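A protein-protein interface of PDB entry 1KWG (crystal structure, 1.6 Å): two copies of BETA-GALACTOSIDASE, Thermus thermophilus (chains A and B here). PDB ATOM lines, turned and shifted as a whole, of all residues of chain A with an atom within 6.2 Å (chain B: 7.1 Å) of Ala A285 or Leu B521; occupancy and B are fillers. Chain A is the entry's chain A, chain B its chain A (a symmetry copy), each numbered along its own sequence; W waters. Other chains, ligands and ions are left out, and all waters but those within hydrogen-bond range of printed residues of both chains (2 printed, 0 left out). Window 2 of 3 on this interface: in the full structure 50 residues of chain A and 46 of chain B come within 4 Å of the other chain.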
ATOM      1  N   LEU A 268     -21.257 -27.638   7.438  1.00  0.00           N
ATOM      2  CA  LEU A 268     -21.321 -26.190   7.252  1.00  0.00           C
ATOM      3  C   LEU A 268     -20.146 -25.466   7.893  1.00  0.00           C
ATOM      4  O   LEU A 268     -19.651 -24.478   7.351  1.00  0.00           O
ATOM      5  CB  LEU A 268     -22.634 -25.630   7.806  1.00  0.00           C
ATOM      6  CG  LEU A 268     -23.918 -26.275   7.273  1.00  0.00           C
ATOM      7  CD1 LEU A 268     -25.099 -25.385   7.636  1.00  0.00           C
ATOM      8  CD2 LEU A 268     -23.842 -26.452   5.760  1.00  0.00           C
ATOM      9  N   THR A 271     -16.959 -26.259   5.821  1.00  0.00           N
ATOM     10  CA  THR A 271     -17.064 -25.548   4.555  1.00  0.00           C
ATOM     11  C   THR A 271     -16.804 -24.048   4.645  1.00  0.00           C
ATOM     12  O   THR A 271     -16.128 -23.486   3.785  1.00  0.00           O
ATOM     13  CB  THR A 271     -18.434 -25.818   3.907  1.00  0.00           C
ATOM     14  OG1 THR A 271     -18.565 -27.229   3.687  1.00  0.00           O
ATOM     15  CG2 THR A 271     -18.555 -25.106   2.564  1.00  0.00           C
ATOM     16  N   GLU A 280     -18.547 -21.008  -5.164  1.00  0.00           N
ATOM     17  CA  GLU A 280     -18.854 -22.185  -4.355  1.00  0.00           C
ATOM     18  C   GLU A 280     -19.130 -21.869  -2.892  1.00  0.00           C
ATOM     19  O   GLU A 280     -19.965 -22.522  -2.268  1.00  0.00           O
ATOM     20  CB  GLU A 280     -17.720 -23.215  -4.427  1.00  0.00           C
ATOM     21  CG  GLU A 280     -17.448 -23.777  -5.813  1.00  0.00           C
ATOM     22  CD  GLU A 280     -16.681 -25.087  -5.765  1.00  0.00           C
ATOM     23  OE1 GLU A 280     -15.815 -25.242  -4.879  1.00  0.00           O
ATOM     24  OE2 GLU A 280     -16.940 -25.963  -6.615  1.00  0.00           O
ATOM     25  N   LYS A 281     -18.435 -20.877  -2.339  1.00  0.00           N
ATOM     26  CA  LYS A 281     -18.632 -20.523  -0.936  1.00  0.00           C
ATOM     27  C   LYS A 281     -20.075 -20.095  -0.690  1.00  0.00           C
ATOM     28  O   LYS A 281     -20.632 -20.343   0.377  1.00  0.00           O
ATOM     29  CB  LYS A 281     -17.669 -19.404  -0.515  1.00  0.00           C
ATOM     30  CG  LYS A 281     -18.017 -18.029  -1.050  1.00  0.00           C
ATOM     31  CD  LYS A 281     -16.903 -17.028  -0.771  1.00  0.00           C
ATOM     32  CE  LYS A 281     -17.299 -15.624  -1.206  1.00  0.00           C
ATOM     33  NZ  LYS A 281     -17.760 -15.567  -2.618  1.00  0.00           N
ATOM     34  N   LEU A 282     -20.686 -19.461  -1.684  1.00  0.00           N
ATOM     35  CA  LEU A 282     -22.068 -19.020  -1.540  1.00  0.00           C
ATOM     36  C   LEU A 282     -23.034 -20.164  -1.832  1.00  0.00           C
ATOM     37  O   LEU A 282     -24.005 -20.375  -1.109  1.00  0.00           O
ATOM     38  CB  LEU A 282     -22.359 -17.850  -2.488  1.00  0.00           C
ATOM     39  CG  LEU A 282     -21.458 -16.622  -2.343  1.00  0.00           C
ATOM     40  CD1 LEU A 282     -21.926 -15.530  -3.297  1.00  0.00           C
ATOM     41  CD2 LEU A 282     -21.490 -16.126  -0.905  1.00  0.00           C
ATOM     42  N   ARG A 283     -22.752 -20.904  -2.897  1.00  0.00           N
ATOM     43  CA  ARG A 283     -23.598 -22.012  -3.309  1.00  0.00           C
ATOM     44  C   ARG A 283     -23.737 -23.108  -2.258  1.00  0.00           C
ATOM     45  O   ARG A 283     -24.818 -23.666  -2.069  1.00  0.00           O
ATOM     46  CB  ARG A 283     -23.048 -22.620  -4.605  1.00  0.00           C
ATOM     47  CG  ARG A 283     -23.831 -23.818  -5.110  1.00  0.00           C
ATOM     48  CD  ARG A 283     -23.248 -24.353  -6.408  1.00  0.00           C
ATOM     49  NE  ARG A 283     -23.974 -25.531  -6.876  1.00  0.00           N
ATOM     50  CZ  ARG A 283     -23.740 -26.144  -8.033  1.00  0.00           C
ATOM     51  NH1 ARG A 283     -22.796 -25.691  -8.849  1.00  0.00           N
ATOM     52  NH2 ARG A 283     -24.450 -27.211  -8.373  1.00  0.00           N
ATOM     53  N   TYR A 284     -22.642 -23.401  -1.566  1.00  0.00           N
ATOM     54  CA  TYR A 284     -22.638 -24.469  -0.572  1.00  0.00           C
ATOM     55  C   TYR A 284     -22.646 -24.014   0.883  1.00  0.00           C
ATOM     56  O   TYR A 284     -22.369 -24.804   1.782  1.00  0.00           O
ATOM     57  CB  TYR A 284     -21.425 -25.375  -0.820  1.00  0.00           C
ATOM     58  CG  TYR A 284     -21.408 -25.990  -2.208  1.00  0.00           C
ATOM     59  CD1 TYR A 284     -22.513 -26.689  -2.690  1.00  0.00           C
ATOM     60  CD2 TYR A 284     -20.288 -25.875  -3.034  1.00  0.00           C
ATOM     61  CE1 TYR A 284     -22.508 -27.260  -3.959  1.00  0.00           C
ATOM     62  CE2 TYR A 284     -20.273 -26.444  -4.308  1.00  0.00           C
ATOM     63  CZ  TYR A 284     -21.388 -27.133  -4.760  1.00  0.00           C
ATOM     64  OH  TYR A 284     -21.394 -27.701  -6.014  1.00  0.00           O
ATOM     65  N   ALA A 285     -22.984 -22.753   1.121  1.00  0.00           N
ATOM     66  CA  ALA A 285     -23.006 -22.229   2.483  1.00  0.00           C
ATOM     67  C   ALA A 285     -23.964 -22.983   3.406  1.00  0.00           C
ATOM     68  O   ALA A 285     -23.670 -23.174   4.590  1.00  0.00           O
ATOM     69  CB  ALA A 285     -23.364 -20.745   2.461  1.00  0.00           C
ATOM     70  N   ARG A 286     -25.099 -23.416   2.865  1.00  0.00           N
ATOM     71  CA  ARG A 286     -26.098 -24.124   3.659  1.00  0.00           C
ATOM     72  C   ARG A 286     -26.154 -25.629   3.406  1.00  0.00           C
ATOM     73  O   ARG A 286     -27.024 -26.324   3.938  1.00  0.00           O
ATOM     74  CB  ARG A 286     -27.483 -23.526   3.404  1.00  0.00           C
ATOM     75  CG  ARG A 286     -27.648 -22.078   3.843  1.00  0.00           C
ATOM     76  CD  ARG A 286     -29.125 -21.733   3.851  1.00  0.00           C
ATOM     77  NE  ARG A 286     -29.439 -20.416   4.402  1.00  0.00           N
ATOM     78  CZ  ARG A 286     -29.585 -19.311   3.679  1.00  0.00           C
ATOM     79  NH1 ARG A 286     -29.429 -19.347   2.360  1.00  0.00           N
ATOM     80  NH2 ARG A 286     -29.950 -18.176   4.267  1.00  0.00           N
ATOM     81  N   THR A 287     -25.223 -26.140   2.608  1.00  0.00           N
ATOM     82  CA  THR A 287     -25.214 -27.565   2.301  1.00  0.00           C
ATOM     83  C   THR A 287     -23.895 -28.233   2.649  1.00  0.00           C
ATOM     84  O   THR A 287     -23.853 -29.429   2.948  1.00  0.00           O
ATOM     85  CB  THR A 287     -25.450 -27.813   0.798  1.00  0.00           C
ATOM     86  OG1 THR A 287     -24.329 -27.311   0.053  1.00  0.00           O
ATOM     87  CG2 THR A 287     -26.719 -27.117   0.331  1.00  0.00           C
ATOM     88  N   GLY A 288     -22.827 -27.443   2.609  1.00  0.00           N
ATOM     89  CA  GLY A 288     -21.494 -27.961   2.843  1.00  0.00           C
ATOM     90  C   GLY A 288     -20.970 -28.324   1.463  1.00  0.00           C
ATOM     91  O   GLY A 288     -21.769 -28.559   0.554  1.00  0.00           O
ATOM     92  N   PRO A 325     -24.488 -20.655   8.979  1.00  0.00           N
ATOM     93  CA  PRO A 325     -25.801 -20.705   8.335  1.00  0.00           C
ATOM     94  C   PRO A 325     -26.600 -21.903   8.827  1.00  0.00           C
ATOM     95  O   PRO A 325     -26.074 -22.787   9.510  1.00  0.00           O
ATOM     96  CB  PRO A 325     -25.459 -20.854   6.850  1.00  0.00           C
ATOM     97  CG  PRO A 325     -24.022 -20.402   6.744  1.00  0.00           C
ATOM     98  CD  PRO A 325     -23.419 -20.942   8.010  1.00  0.00           C
ATOM     99  N   SER A 326     -27.877 -21.928   8.483  1.00  0.00           N
ATOM    100  CA  SER A 326     -28.707 -23.062   8.840  1.00  0.00           C
ATOM    101  C   SER A 326     -28.608 -24.059   7.700  1.00  0.00           C
ATOM    102  O   SER A 326     -28.458 -23.669   6.541  1.00  0.00           O
ATOM    103  CB  SER A 326     -30.172 -22.656   8.974  1.00  0.00           C
ATOM    104  OG  SER A 326     -31.001 -23.810   8.929  1.00  0.00           O
ATOM    105  N   GLU B 515     -29.289 -17.309  11.725  1.00  0.00           N
ATOM    106  CA  GLU B 515     -28.235 -17.675  10.783  1.00  0.00           C
ATOM    107  C   GLU B 515     -27.286 -16.510  10.564  1.00  0.00           C
ATOM    108  O   GLU B 515     -27.725 -15.364  10.466  1.00  0.00           O
ATOM    109  CB  GLU B 515     -28.794 -17.979   9.386  1.00  0.00           C
ATOM    110  CG  GLU B 515     -29.931 -18.960   9.254  1.00  0.00           C
ATOM    111  CD  GLU B 515     -30.196 -19.261   7.786  1.00  0.00           C
ATOM    112  OE1 GLU B 515     -29.339 -19.923   7.164  1.00  0.00           O
ATOM    113  OE2 GLU B 515     -31.236 -18.820   7.250  1.00  0.00           O
ATOM    114  N   SER B 516     -25.990 -16.800  10.497  1.00  0.00           N
ATOM    115  CA  SER B 516     -25.021 -15.774  10.141  1.00  0.00           C
ATOM    116  C   SER B 516     -24.559 -16.311   8.782  1.00  0.00           C
ATOM    117  O   SER B 516     -24.321 -17.518   8.619  1.00  0.00           O
ATOM    118  CB  SER B 516     -23.878 -15.648  11.161  1.00  0.00           C
ATOM    119  OG  SER B 516     -23.194 -16.856  11.398  1.00  0.00           O
ATOM    120  N   LEU B 517     -24.480 -15.420   7.800  1.00  0.00           N
ATOM    121  CA  LEU B 517     -24.147 -15.798   6.434  1.00  0.00           C
ATOM    122  C   LEU B 517     -22.883 -15.144   5.894  1.00  0.00           C
ATOM    123  O   LEU B 517     -22.569 -14.004   6.237  1.00  0.00           O
ATOM    124  CB  LEU B 517     -25.328 -15.432   5.532  1.00  0.00           C
ATOM    125  CG  LEU B 517     -26.699 -15.943   5.992  1.00  0.00           C
ATOM    126  CD1 LEU B 517     -27.812 -15.217   5.248  1.00  0.00           C
ATOM    127  CD2 LEU B 517     -26.784 -17.436   5.761  1.00  0.00           C
ATOM    128  N   PRO B 518     -22.149 -15.856   5.020  1.00  0.00           N
ATOM    129  CA  PRO B 518     -20.918 -15.314   4.444  1.00  0.00           C
ATOM    130  C   PRO B 518     -21.191 -14.081   3.586  1.00  0.00           C
ATOM    131  O   PRO B 518     -22.256 -13.956   2.979  1.00  0.00           O
ATOM    132  CB  PRO B 518     -20.376 -16.488   3.626  1.00  0.00           C
ATOM    133  CG  PRO B 518     -21.628 -17.194   3.185  1.00  0.00           C
ATOM    134  CD  PRO B 518     -22.458 -17.183   4.454  1.00  0.00           C
ATOM    135  N   PRO B 519     -20.237 -13.143   3.544  1.00  0.00           N
ATOM    136  CA  PRO B 519     -20.436 -11.939   2.737  1.00  0.00           C
ATOM    137  C   PRO B 519     -20.723 -12.306   1.286  1.00  0.00           C
ATOM    138  O   PRO B 519     -20.077 -13.190   0.716  1.00  0.00           O
ATOM    139  CB  PRO B 519     -19.118 -11.177   2.914  1.00  0.00           C
ATOM    140  CG  PRO B 519     -18.124 -12.255   3.245  1.00  0.00           C
ATOM    141  CD  PRO B 519     -18.908 -13.144   4.178  1.00  0.00           C
ATOM    142  N   GLY B 520     -21.710 -11.641   0.697  1.00  0.00           N
ATOM    143  CA  GLY B 520     -22.056 -11.928  -0.681  1.00  0.00           C
ATOM    144  C   GLY B 520     -23.302 -12.777  -0.835  1.00  0.00           C
ATOM    145  O   GLY B 520     -23.918 -12.784  -1.902  1.00  0.00           O
ATOM    146  N   LEU B 521     -23.679 -13.509   0.213  1.00  0.00           N
ATOM    147  CA  LEU B 521     -24.875 -14.341   0.139  1.00  0.00           C
ATOM    148  C   LEU B 521     -26.085 -13.471   0.463  1.00  0.00           C
ATOM    149  O   LEU B 521     -26.354 -13.155   1.624  1.00  0.00           O
ATOM    150  CB  LEU B 521     -24.784 -15.518   1.120  1.00  0.00           C
ATOM    151  CG  LEU B 521     -25.673 -16.729   0.793  1.00  0.00           C
ATOM    152  CD1 LEU B 521     -25.333 -17.883   1.725  1.00  0.00           C
ATOM    153  CD2 LEU B 521     -27.138 -16.358   0.914  1.00  0.00           C
ATOM    154  N   LEU B 522     -26.808 -13.073  -0.577  1.00  0.00           N
ATOM    155  CA  LEU B 522     -27.974 -12.219  -0.413  1.00  0.00           C
ATOM    156  C   LEU B 522     -29.254 -12.897  -0.877  1.00  0.00           C
ATOM    157  O   LEU B 522     -29.234 -13.762  -1.753  1.00  0.00           O
ATOM    158  CB  LEU B 522     -27.787 -10.924  -1.213  1.00  0.00           C
ATOM    159  CG  LEU B 522     -26.534 -10.098  -0.930  1.00  0.00           C
ATOM    160  CD1 LEU B 522     -26.448  -8.944  -1.919  1.00  0.00           C
ATOM    161  CD2 LEU B 522     -26.573  -9.580   0.498  1.00  0.00           C
ATOM    162  N   GLU B 523     -30.366 -12.504  -0.268  1.00  0.00           N
ATOM    163  CA  GLU B 523     -31.675 -13.024  -0.634  1.00  0.00           C
ATOM    164  C   GLU B 523     -32.656 -11.870  -0.513  1.00  0.00           C
ATOM    165  O   GLU B 523     -32.629 -11.112   0.458  1.00  0.00           O
ATOM    166  CB  GLU B 523     -32.112 -14.171   0.282  1.00  0.00           C
ATOM    167  CG  GLU B 523     -33.312 -14.933  -0.274  1.00  0.00           C
ATOM    168  CD  GLU B 523     -33.807 -16.039   0.639  1.00  0.00           C
ATOM    169  OE1 GLU B 523     -32.965 -16.746   1.235  1.00  0.00           O
ATOM    170  OE2 GLU B 523     -35.039 -16.212   0.749  1.00  0.00           O
ATOM    171  N   PRO B 533     -32.401  -6.860  -1.133  1.00  0.00           N
ATOM    172  CA  PRO B 533     -31.512  -8.017  -1.021  1.00  0.00           C
ATOM    173  C   PRO B 533     -30.857  -7.872   0.351  1.00  0.00           C
ATOM    174  O   PRO B 533     -30.247  -6.840   0.640  1.00  0.00           O
ATOM    175  CB  PRO B 533     -30.510  -7.802  -2.155  1.00  0.00           C
ATOM    176  CG  PRO B 533     -31.303  -7.017  -3.170  1.00  0.00           C
ATOM    177  CD  PRO B 533     -32.041  -6.029  -2.295  1.00  0.00           C
ATOM    178  N   LEU B 534     -30.997  -8.886   1.197  1.00  0.00           N
ATOM    179  CA  LEU B 534     -30.426  -8.829   2.538  1.00  0.00           C
ATOM    180  C   LEU B 534     -29.509 -10.016   2.808  1.00  0.00           C
ATOM    181  O   LEU B 534     -29.644 -11.074   2.191  1.00  0.00           O
ATOM    182  CB  LEU B 534     -31.547  -8.804   3.583  1.00  0.00           C
ATOM    183  CG  LEU B 534     -32.591  -7.688   3.472  1.00  0.00           C
ATOM    184  CD1 LEU B 534     -33.681  -7.894   4.518  1.00  0.00           C
ATOM    185  CD2 LEU B 534     -31.927  -6.338   3.662  1.00  0.00           C
ATOM    186  N   GLY B 535     -28.577  -9.837   3.738  1.00  0.00           N
ATOM    187  CA  GLY B 535     -27.665 -10.913   4.078  1.00  0.00           C
ATOM    188  C   GLY B 535     -27.112 -10.724   5.477  1.00  0.00           C
ATOM    189  O   GLY B 535     -27.750 -10.082   6.309  1.00  0.00           O
ATOM    190  N   LEU B 536     -25.940 -11.305   5.724  1.00  0.00           N
ATOM    191  CA  LEU B 536     -25.218 -11.205   6.997  1.00  0.00           C
ATOM    192  C   LEU B 536     -25.858 -11.896   8.198  1.00  0.00           C
ATOM    193  O   LEU B 536     -25.230 -12.753   8.828  1.00  0.00           O
ATOM    194  CB  LEU B 536     -24.951  -9.728   7.331  1.00  0.00           C
ATOM    195  CG  LEU B 536     -23.884  -9.424   8.394  1.00  0.00           C
ATOM    196  CD1 LEU B 536     -23.377  -7.997   8.214  1.00  0.00           C
ATOM    197  CD2 LEU B 536     -24.457  -9.615   9.796  1.00  0.00           C
ATOM    198  N   ARG B 538     -29.783 -13.494   9.546  1.00  0.00           N
ATOM    199  CA  ARG B 538     -31.169 -13.804   9.242  1.00  0.00           C
ATOM    200  C   ARG B 538     -31.769 -14.636  10.364  1.00  0.00           C
ATOM    201  O   ARG B 538     -31.134 -15.559  10.868  1.00  0.00           O
ATOM    202  CB  ARG B 538     -31.263 -14.563   7.920  1.00  0.00           C
ATOM    203  CG  ARG B 538     -32.675 -14.921   7.546  1.00  0.00           C
ATOM    204  CD  ARG B 538     -32.750 -15.512   6.161  1.00  0.00           C
ATOM    205  NE  ARG B 538     -34.115 -15.910   5.854  1.00  0.00           N
ATOM    206  CZ  ARG B 538     -34.496 -16.430   4.697  1.00  0.00           C
ATOM    207  NH1 ARG B 538     -33.611 -16.617   3.729  1.00  0.00           N
ATOM    208  NH2 ARG B 538     -35.763 -16.759   4.513  1.00  0.00           N
HETATM  209  O   HOH W   1     -30.684 -17.641   0.362  1.00  0.00           O
HETATM  210  O   HOH W   2     -30.850 -15.827   2.857  1.00  0.00           O
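Printed residues of chain A that touch a printed residue of chain B: Leu A282, Ala A285, Arg A286, Pro A325 and Ser A326.
Of the 14 printed residues of chain B, 6 touch a printed residue of chain A.
Among the printed residues, Asp or Glu carboxylates within 4 Å of a Lys or Arg side-chain nitrogen of the other chain: Arg A286 with Glu B515 (2.8 Å).
Water W1 bridges the side-chain carboxylate (OE1) of Glu B523 (2.6 Å) and the guanidinium group (NH1) of Arg A286 (2.9 Å).
Water W2 lies within hydrogen-bond range of the side-chain carboxylate of Glu B523 (2.8 Å), the guanidinium group of Arg A286 (2.9 Å) and the guanidinium group of Arg B538 (3.0 Å).
N of Leu B517 is in hydrogen-bond range of O of Leu B536, at 3.0 Å.
N of Glu B515 lies within hydrogen-bond range of O of Arg B538 (2.7 Å).
The backbone NH of Ser A326 is in hydrogen-bond range of the side-chain carboxylate of Glu B515 (2.8 Å).
OE1 of Glu B515 is in salt-bridge range of NE of Arg A286.
The backbone carbonyl oxygen of Ser B516 lies close to the backbone nitrogen of Pro A325.
Printed residues of chain B within 4 Å of Ala A285: Leu B521 (3.6 Å).
Of the printed residues of chain A, Gly B520 touches Leu A282.
Printed residues of chain B within 4 Å of Arg A286: Glu B515 (2.8 Å) and Leu B517 (3.6 Å).
Of the printed residues of chain A, Pro B519 touches Leu A282 (3.6 Å).
Of the printed residues of chain A, Ser B516 touches Pro A325 (3.2 Å).
Printed residues of chain A within 4 Å of Leu B517: Arg A286 (3.6 Å) and Pro A325 (3.8 Å).
Gly A288 touches none of the printed residues of chain B.
The nearest printed residue of chain A that does not touch Pro B519 is Lys A281 (4.2 Å).
Among the printed residues, merely in contact across the chains: Ala A285 with Leu B521, Arg A286 with Leu B517, Leu A282 with Leu B521, Leu A282 with Pro B519, Leu A282 with Gly B520, Pro A325 with Glu B515 and Pro A325 with Leu B517.
No position is printed for both chains.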
